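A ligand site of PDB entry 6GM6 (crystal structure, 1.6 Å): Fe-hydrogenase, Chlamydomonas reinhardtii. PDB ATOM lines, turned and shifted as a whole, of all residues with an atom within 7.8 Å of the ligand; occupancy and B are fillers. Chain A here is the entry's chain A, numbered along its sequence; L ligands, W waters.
A sulfur (S3) of the ligand sits close to the backbone NH (N) of Ala 361, 3.7 Å away. NE of Arg 172 lies close to S4 of the ligand, 3.4 Å away. The side-chain sulfur (SG) of Cys 115 binds an iron atom (FE1) of the ligand (2.3 Å). An iron atom (FE4) of the ligand is bound by the side-chain sulfur (SG) of Cys 366 (2.3 Å). The backbone NH of Cys 362 sits close to a sulfur (S3) of the ligand (3.5 Å). The side-chain sulfur (SG) of Cys 362 binds an iron atom (FE2) of the ligand, 2.3 Å away. FE3 of the ligand is bound by SG of Cys 170 (2.3 Å).
Water W1 lies within hydrogen-bond range of the backbone carbonyl oxygen (O) of Cys 114 (3.2 Å), a sulfur (S2) of the ligand (3.4 Å) and the side-chain amino group (NZ) of Lys 173 (3.4 Å).
The side-chain sulfur (SG) of Cys 115 sits close to the backbone NH (N) of Gly 117 (3.4 Å). SG of Cys 170 sits close to N of Arg 172 (3.3 Å). NZ of Lys 173 lies within salt-bridge range of OE1 of Glu 176 (2.8 Å). N of Met 360 is in hydrogen-bond range of O of Ala 334, at 2.9 Å. The side-chain amide oxygen (OD1) of Asn 335 sits close to the backbone carbonyl oxygen (O) of Cys 362 (3.2 Å). SG of Cys 115 sits close to N of Trp 118 (3.6 Å). N of Lys 173 lies close to SG of Cys 170. O of Cys 114 sits at hydrogen-bond distance from NZ of Lys 173 (2.8 Å).
Residues that only touch the ligand: Pro 116, Lys 173, Met 360 and Gly 369. Hydrophobic or aromatic side chains within 4 Å of the ligand: Pro 116, Met 360 and Ala 361. Within 4 Å of the ligand: Cys 115, Pro 116, Cys 170, Arg 172, Lys 173, Met 360, Ala 361, Cys 362, Cys 366 and Gly 369.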
ATOM      1  N   ALA A  39     -17.506 -12.639  -1.525  1.00  0.00           N
ATOM      2  CA  ALA A  39     -17.730 -12.282  -0.121  1.00  0.00           C
ATOM      3  C   ALA A  39     -18.881 -13.078   0.494  1.00  0.00           C
ATOM      4  O   ALA A  39     -18.882 -13.356   1.688  1.00  0.00           O
ATOM      5  CB  ALA A  39     -17.993 -10.760   0.021  1.00  0.00           C
ATOM      6  N   CYS A 114     -17.880   0.521  -8.898  1.00  0.00           N
ATOM      7  CA  CYS A 114     -18.536  -0.738  -8.551  1.00  0.00           C
ATOM      8  C   CYS A 114     -19.335  -0.684  -7.247  1.00  0.00           C
ATOM      9  O   CYS A 114     -20.184  -1.538  -7.016  1.00  0.00           O
ATOM     10  CB  CYS A 114     -17.493  -1.859  -8.458  1.00  0.00           C
ATOM     11  SG  CYS A 114     -16.128  -1.545  -7.333  1.00  0.00           S
ATOM     12  N   CYS A 115     -19.065   0.315  -6.400  1.00  0.00           N
ATOM     13  CA  CYS A 115     -19.810   0.429  -5.135  1.00  0.00           C
ATOM     14  C   CYS A 115     -21.010   1.361  -5.292  1.00  0.00           C
ATOM     15  O   CYS A 115     -20.835   2.558  -5.528  1.00  0.00           O
ATOM     16  CB  CYS A 115     -18.912   0.950  -4.005  1.00  0.00           C
ATOM     17  SG  CYS A 115     -19.832   1.185  -2.430  1.00  0.00           S
ATOM     18  N   PRO A 116     -22.231   0.827  -5.133  1.00  0.00           N
ATOM     19  CA  PRO A 116     -23.396   1.716  -5.323  1.00  0.00           C
ATOM     20  C   PRO A 116     -23.524   2.778  -4.231  1.00  0.00           C
ATOM     21  O   PRO A 116     -24.167   3.795  -4.492  1.00  0.00           O
ATOM     22  CB  PRO A 116     -24.600   0.759  -5.309  1.00  0.00           C
ATOM     23  CG  PRO A 116     -24.084  -0.560  -4.827  1.00  0.00           C
ATOM     24  CD  PRO A 116     -22.590  -0.589  -4.946  1.00  0.00           C
ATOM     25  N   GLY A 117     -22.926   2.575  -3.060  1.00  0.00           N
ATOM     26  CA  GLY A 117     -22.925   3.615  -2.041  1.00  0.00           C
ATOM     27  C   GLY A 117     -22.119   4.820  -2.483  1.00  0.00           C
ATOM     28  O   GLY A 117     -22.492   5.982  -2.246  1.00  0.00           O
ATOM     29  N   TRP A 118     -21.004   4.548  -3.155  1.00  0.00           N
ATOM     30  CA  TRP A 118     -20.198   5.621  -3.741  1.00  0.00           C
ATOM     31  C   TRP A 118     -20.963   6.309  -4.869  1.00  0.00           C
ATOM     32  O   TRP A 118     -21.021   7.536  -4.929  1.00  0.00           O
ATOM     33  CB  TRP A 118     -18.844   5.066  -4.238  1.00  0.00           C
ATOM     34  CG  TRP A 118     -18.143   5.860  -5.326  1.00  0.00           C
ATOM     35  CD1 TRP A 118     -17.641   5.346  -6.504  1.00  0.00           C
ATOM     36  CD2 TRP A 118     -17.855   7.271  -5.349  1.00  0.00           C
ATOM     37  NE1 TRP A 118     -17.076   6.359  -7.251  1.00  0.00           N
ATOM     38  CE2 TRP A 118     -17.194   7.546  -6.566  1.00  0.00           C
ATOM     39  CE3 TRP A 118     -18.096   8.318  -4.465  1.00  0.00           C
ATOM     40  CZ2 TRP A 118     -16.766   8.829  -6.919  1.00  0.00           C
ATOM     41  CZ3 TRP A 118     -17.692   9.597  -4.819  1.00  0.00           C
ATOM     42  CH2 TRP A 118     -17.021   9.836  -6.032  1.00  0.00           C
ATOM     43  N   SER A 138     -20.864  -2.623 -12.789  1.00  0.00           N
ATOM     44  CA  SER A 138     -20.280  -3.537 -11.809  1.00  0.00           C
ATOM     45  C   SER A 138     -20.147  -4.969 -12.336  1.00  0.00           C
ATOM     46  O   SER A 138     -20.772  -5.326 -13.327  1.00  0.00           O
ATOM     47  CB  SER A 138     -21.159  -3.567 -10.555  1.00  0.00           C
ATOM     48  OG  SER A 138     -22.361  -4.245 -10.885  1.00  0.00           O
ATOM     49  N   MET A 168     -25.397 -11.280  -2.804  1.00  0.00           N
ATOM     50  CA  MET A 168     -24.424 -10.228  -2.525  1.00  0.00           C
ATOM     51  C   MET A 168     -24.250 -10.010  -1.031  1.00  0.00           C
ATOM     52  O   MET A 168     -25.144 -10.320  -0.242  1.00  0.00           O
ATOM     53  CB  MET A 168     -24.885  -8.902  -3.162  1.00  0.00           C
ATOM     54  CG  MET A 168     -24.875  -8.928  -4.664  1.00  0.00           C
ATOM     55  SD  MET A 168     -23.138  -8.826  -5.269  1.00  0.00           S
ATOM     56  CE  MET A 168     -23.188 -10.027  -6.561  1.00  0.00           C
ATOM     57  N   PRO A 169     -23.092  -9.457  -0.633  1.00  0.00           N
ATOM     58  CA  PRO A 169     -22.858  -9.127   0.780  1.00  0.00           C
ATOM     59  C   PRO A 169     -23.424  -7.773   1.151  1.00  0.00           C
ATOM     60  O   PRO A 169     -23.194  -7.276   2.252  1.00  0.00           O
ATOM     61  CB  PRO A 169     -21.320  -9.102   0.860  1.00  0.00           C
ATOM     62  CG  PRO A 169     -20.945  -8.526  -0.479  1.00  0.00           C
ATOM     63  CD  PRO A 169     -21.878  -9.250  -1.444  1.00  0.00           C
ATOM     64  N   CYS A 170     -24.180  -7.206   0.233  1.00  0.00           N
ATOM     65  CA  CYS A 170     -24.411  -5.767   0.174  1.00  0.00           C
ATOM     66  C   CYS A 170     -25.905  -5.454   0.177  1.00  0.00           C
ATOM     67  O   CYS A 170     -26.659  -6.085  -0.536  1.00  0.00           O
ATOM     68  CB  CYS A 170     -23.751  -5.224  -1.095  1.00  0.00           C
ATOM     69  SG  CYS A 170     -23.955  -3.476  -1.310  1.00  0.00           S
ATOM     70  N   THR A 171     -26.323  -4.480   0.979  1.00  0.00           N
ATOM     71  CA  THR A 171     -27.714  -4.066   1.029  1.00  0.00           C
ATOM     72  C   THR A 171     -28.066  -2.995   0.005  1.00  0.00           C
ATOM     73  O   THR A 171     -29.207  -2.530  -0.040  1.00  0.00           O
ATOM     74  CB  THR A 171     -28.076  -3.523   2.418  1.00  0.00           C
ATOM     75  OG1 THR A 171     -27.157  -2.477   2.769  1.00  0.00           O
ATOM     76  CG2 THR A 171     -28.017  -4.634   3.455  1.00  0.00           C
ATOM     77  N   ARG A 172     -27.092  -2.610  -0.820  1.00  0.00           N
ATOM     78  CA  ARG A 172     -27.270  -1.546  -1.815  1.00  0.00           C
ATOM     79  C   ARG A 172     -27.294  -2.081  -3.245  1.00  0.00           C
ATOM     80  O   ARG A 172     -27.504  -1.327  -4.200  1.00  0.00           O
ATOM     81  CB  ARG A 172     -26.150  -0.517  -1.701  1.00  0.00           C
ATOM     82  CG  ARG A 172     -25.916   0.057  -0.290  1.00  0.00           C
ATOM     83  CD  ARG A 172     -24.888   1.184  -0.388  1.00  0.00           C
ATOM     84  NE  ARG A 172     -24.169   1.463   0.857  1.00  0.00           N
ATOM     85  CZ  ARG A 172     -24.278   2.610   1.523  1.00  0.00           C
ATOM     86  NH1 ARG A 172     -25.081   3.563   1.082  1.00  0.00           N
ATOM     87  NH2 ARG A 172     -23.571   2.799   2.635  1.00  0.00           N
ATOM     88  N   LYS A 173     -27.031  -3.369  -3.428  1.00  0.00           N
ATOM     89  CA  LYS A 173     -26.863  -3.884  -4.781  1.00  0.00           C
ATOM     90  C   LYS A 173     -28.198  -3.998  -5.526  1.00  0.00           C
ATOM     91  O   LYS A 173     -28.216  -3.961  -6.755  1.00  0.00           O
ATOM     92  CB  LYS A 173     -26.127  -5.234  -4.752  1.00  0.00           C
ATOM     93  CG  LYS A 173     -24.594  -5.061  -4.625  1.00  0.00           C
ATOM     94  CD  LYS A 173     -23.961  -4.565  -5.934  1.00  0.00           C
ATOM     95  CE  LYS A 173     -22.471  -4.232  -5.726  1.00  0.00           C
ATOM     96  NZ  LYS A 173     -21.851  -3.804  -7.006  1.00  0.00           N
ATOM     97  N   GLU A 176     -28.586  -0.681  -7.203  1.00  0.00           N
ATOM     98  CA  GLU A 176     -27.769  -0.688  -8.417  1.00  0.00           C
ATOM     99  C   GLU A 176     -28.518  -1.380  -9.556  1.00  0.00           C
ATOM    100  O   GLU A 176     -28.635  -0.832 -10.659  1.00  0.00           O
ATOM    101  CB  GLU A 176     -26.444  -1.391  -8.153  1.00  0.00           C
ATOM    102  CG  GLU A 176     -25.504  -1.506  -9.351  1.00  0.00           C
ATOM    103  CD  GLU A 176     -24.305  -2.355  -9.020  1.00  0.00           C
ATOM    104  OE1 GLU A 176     -23.344  -1.842  -8.409  1.00  0.00           O
ATOM    105  OE2 GLU A 176     -24.343  -3.570  -9.332  1.00  0.00           O
ATOM    106  N   ALA A 334     -10.078   4.402  -0.842  1.00  0.00           N
ATOM    107  CA  ALA A 334     -10.797   4.955   0.305  1.00  0.00           C
ATOM    108  C   ALA A 334     -11.878   3.975   0.744  1.00  0.00           C
ATOM    109  O   ALA A 334     -12.663   3.529  -0.083  1.00  0.00           O
ATOM    110  CB  ALA A 334     -11.419   6.284  -0.038  1.00  0.00           C
ATOM    111  N   ASN A 335     -11.901   3.645   2.035  1.00  0.00           N
ATOM    112  CA  ASN A 335     -12.963   2.839   2.603  1.00  0.00           C
ATOM    113  C   ASN A 335     -13.733   3.658   3.629  1.00  0.00           C
ATOM    114  O   ASN A 335     -13.127   4.208   4.549  1.00  0.00           O
ATOM    115  CB  ASN A 335     -12.399   1.582   3.250  1.00  0.00           C
ATOM    116  CG  ASN A 335     -12.023   0.525   2.236  1.00  0.00           C
ATOM    117  OD1 ASN A 335     -12.846  -0.314   1.857  1.00  0.00           O
ATOM    118  ND2 ASN A 335     -10.788   0.575   1.768  1.00  0.00           N
ATOM    119  N   GLY A 336     -15.048   3.720   3.459  1.00  0.00           N
ATOM    120  CA  GLY A 336     -15.902   4.570   4.279  1.00  0.00           C
ATOM    121  C   GLY A 336     -16.216   5.854   3.541  1.00  0.00           C
ATOM    122  O   GLY A 336     -15.307   6.566   3.109  1.00  0.00           O
ATOM    123  N   LEU A 337     -17.497   6.184   3.409  1.00  0.00           N
ATOM    124  CA  LEU A 337     -17.879   7.358   2.629  1.00  0.00           C
ATOM    125  C   LEU A 337     -17.444   8.658   3.305  1.00  0.00           C
ATOM    126  O   LEU A 337     -17.176   9.641   2.623  1.00  0.00           O
ATOM    127  CB  LEU A 337     -19.380   7.373   2.357  1.00  0.00           C
ATOM    128  CG  LEU A 337     -19.883   6.242   1.460  1.00  0.00           C
ATOM    129  CD1 LEU A 337     -21.398   6.289   1.325  1.00  0.00           C
ATOM    130  CD2 LEU A 337     -19.211   6.294   0.070  1.00  0.00           C
ATOM    131  N   ILE A 359     -13.312   4.057  -4.421  1.00  0.00           N
ATOM    132  CA  ILE A 359     -14.070   4.427  -3.229  1.00  0.00           C
ATOM    133  C   ILE A 359     -15.087   3.346  -2.907  1.00  0.00           C
ATOM    134  O   ILE A 359     -15.899   2.987  -3.759  1.00  0.00           O
ATOM    135  CB  ILE A 359     -14.783   5.789  -3.408  1.00  0.00           C
ATOM    136  CG1 ILE A 359     -13.755   6.905  -3.546  1.00  0.00           C
ATOM    137  CG2 ILE A 359     -15.704   6.051  -2.223  1.00  0.00           C
ATOM    138  CD1 ILE A 359     -14.358   8.249  -3.963  1.00  0.00           C
ATOM    139  N   MET A 360     -14.994   2.797  -1.698  1.00  0.00           N
ATOM    140  CA  MET A 360     -15.920   1.764  -1.237  1.00  0.00           C
ATOM    141  C   MET A 360     -16.606   2.258   0.024  1.00  0.00           C
ATOM    142  O   MET A 360     -15.947   2.802   0.917  1.00  0.00           O
ATOM    143  CB  MET A 360     -15.217   0.425  -0.975  1.00  0.00           C
ATOM    144  CG  MET A 360     -14.362  -0.116  -2.126  1.00  0.00           C
ATOM    145  SD  MET A 360     -15.277  -0.604  -3.612  1.00  0.00           S
ATOM    146  CE  MET A 360     -16.068  -2.105  -3.067  1.00  0.00           C
ATOM    147  N   ALA A 361     -17.912   2.043   0.135  1.00  0.00           N
ATOM    148  CA  ALA A 361     -18.659   2.644   1.243  1.00  0.00           C
ATOM    149  C   ALA A 361     -18.372   1.952   2.584  1.00  0.00           C
ATOM    150  O   ALA A 361     -18.371   2.602   3.633  1.00  0.00           O
ATOM    151  CB  ALA A 361     -20.161   2.617   0.933  1.00  0.00           C
ATOM    152  N   CYS A 362     -18.128   0.649   2.559  1.00  0.00           N
ATOM    153  CA  CYS A 362     -17.927  -0.085   3.810  1.00  0.00           C
ATOM    154  C   CYS A 362     -16.491   0.040   4.296  1.00  0.00           C
ATOM    155  O   CYS A 362     -15.550  -0.108   3.510  1.00  0.00           O
ATOM    156  CB  CYS A 362     -18.314  -1.554   3.659  1.00  0.00           C
ATOM    157  SG  CYS A 362     -20.069  -1.783   3.256  1.00  0.00           S
ATOM    158  N   PRO A 363     -16.316   0.320   5.589  1.00  0.00           N
ATOM    159  CA  PRO A 363     -14.982   0.413   6.210  1.00  0.00           C
ATOM    160  C   PRO A 363     -14.103  -0.784   5.883  1.00  0.00           C
ATOM    161  O   PRO A 363     -12.912  -0.603   5.605  1.00  0.00           O
ATOM    162  CB  PRO A 363     -15.309   0.461   7.713  1.00  0.00           C
ATOM    163  CG  PRO A 363     -16.627   1.156   7.761  1.00  0.00           C
ATOM    164  CD  PRO A 363     -17.382   0.652   6.555  1.00  0.00           C
ATOM    165  N   ALA A 364     -14.669  -1.983   5.877  1.00  0.00           N
ATOM    166  CA  ALA A 364     -13.873  -3.168   5.585  1.00  0.00           C
ATOM    167  C   ALA A 364     -14.005  -3.651   4.134  1.00  0.00           C
ATOM    168  O   ALA A 364     -13.480  -4.702   3.780  1.00  0.00           O
ATOM    169  CB  ALA A 364     -14.243  -4.295   6.547  1.00  0.00           C
ATOM    170  N   GLY A 365     -14.712  -2.887   3.313  1.00  0.00           N
ATOM    171  CA  GLY A 365     -14.981  -3.342   1.965  1.00  0.00           C
ATOM    172  C   GLY A 365     -16.066  -4.409   2.008  1.00  0.00           C
ATOM    173  O   GLY A 365     -16.687  -4.617   3.054  1.00  0.00           O
ATOM    174  N   CYS A 366     -16.259  -5.100   0.886  1.00  0.00           N
ATOM    175  CA  CYS A 366     -17.453  -5.940   0.728  1.00  0.00           C
ATOM    176  C   CYS A 366     -17.505  -7.107   1.716  1.00  0.00           C
ATOM    177  O   CYS A 366     -18.592  -7.537   2.085  1.00  0.00           O
ATOM    178  CB  CYS A 366     -17.555  -6.456  -0.703  1.00  0.00           C
ATOM    179  SG  CYS A 366     -17.800  -5.157  -1.930  1.00  0.00           S
ATOM    180  N   VAL A 367     -16.361  -7.612   2.158  1.00  0.00           N
ATOM    181  CA  VAL A 367     -16.404  -8.697   3.149  1.00  0.00           C
ATOM    182  C   VAL A 367     -17.079  -8.222   4.433  1.00  0.00           C
ATOM    183  O   VAL A 367     -17.583  -9.030   5.193  1.00  0.00           O
ATOM    184  CB  VAL A 367     -15.013  -9.266   3.489  1.00  0.00           C
ATOM    185  CG1 VAL A 367     -14.467 -10.113   2.329  1.00  0.00           C
ATOM    186  CG2 VAL A 367     -14.054  -8.154   3.880  1.00  0.00           C
ATOM    187  N   GLY A 368     -17.118  -6.900   4.647  1.00  0.00           N
ATOM    188  CA  GLY A 368     -17.846  -6.363   5.780  1.00  0.00           C
ATOM    189  C   GLY A 368     -19.122  -5.623   5.411  1.00  0.00           C
ATOM    190  O   GLY A 368     -19.570  -4.727   6.129  1.00  0.00           O
ATOM    191  N   GLY A 369     -19.739  -6.023   4.294  1.00  0.00           N
ATOM    192  CA  GLY A 369     -20.956  -5.387   3.820  1.00  0.00           C
ATOM    193  C   GLY A 369     -22.172  -5.521   4.720  1.00  0.00           C
ATOM    194  O   GLY A 369     -22.229  -6.367   5.620  1.00  0.00           O
ATOM    195  N   GLY A 370     -23.180  -4.707   4.434  1.00  0.00           N
ATOM    196  CA  GLY A 370     -24.346  -4.634   5.304  1.00  0.00           C
ATOM    197  C   GLY A 370     -25.253  -5.854   5.283  1.00  0.00           C
ATOM    198  O   GLY A 370     -26.109  -5.992   6.154  1.00  0.00           O
ATOM    199  N   GLY A 371     -25.080  -6.710   4.258  1.00  0.00           N
ATOM    200  CA  GLY A 371     -25.847  -7.944   4.161  1.00  0.00           C
ATOM    201  C   GLY A 371     -25.126  -9.149   4.750  1.00  0.00           C
ATOM    202  O   GLY A 371     -25.643 -10.273   4.653  1.00  0.00           O
ATOM    203  N   GLN A 372     -23.977  -8.920   5.383  1.00  0.00           N
ATOM    204  CA  GLN A 372     -23.192 -10.006   5.984  1.00  0.00           C
ATOM    205  C   GLN A 372     -23.680 -10.383   7.395  1.00  0.00           C
ATOM    206  O   GLN A 372     -24.295  -9.569   8.094  1.00  0.00           O
ATOM    207  CB  GLN A 372     -21.701  -9.618   6.059  1.00  0.00           C
ATOM    208  CG  GLN A 372     -21.039  -9.393   4.704  1.00  0.00           C
ATOM    209  CD  GLN A 372     -20.788 -10.688   3.947  1.00  0.00           C
ATOM    210  OE1 GLN A 372     -21.721 -11.407   3.574  1.00  0.00           O
ATOM    211  NE2 GLN A 372     -19.509 -10.996   3.711  1.00  0.00           N
HETATM  212 FE1  LIG L   1     -19.978  -0.902  -1.448  1.00  0.00          FE
HETATM  213 FE2  LIG L   1     -20.212  -2.116   0.994  1.00  0.00          FE
HETATM  214 FE3  LIG L   1     -21.779  -2.817  -1.073  1.00  0.00          FE
HETATM  215 FE4  LIG L   1     -19.154  -3.487  -1.152  1.00  0.00          FE
HETATM  216  S1  LIG L   1     -20.737  -4.262   0.349  1.00  0.00           S
HETATM  217  S2  LIG L   1     -20.364  -2.643  -2.883  1.00  0.00           S
HETATM  218  S3  LIG L   1     -18.258  -1.624  -0.126  1.00  0.00           S
HETATM  219  S4  LIG L   1     -21.759  -0.807  -0.050  1.00  0.00           S
HETATM  220  O   HOH W   1     -18.728  -4.035  -5.561  1.00  0.00           O
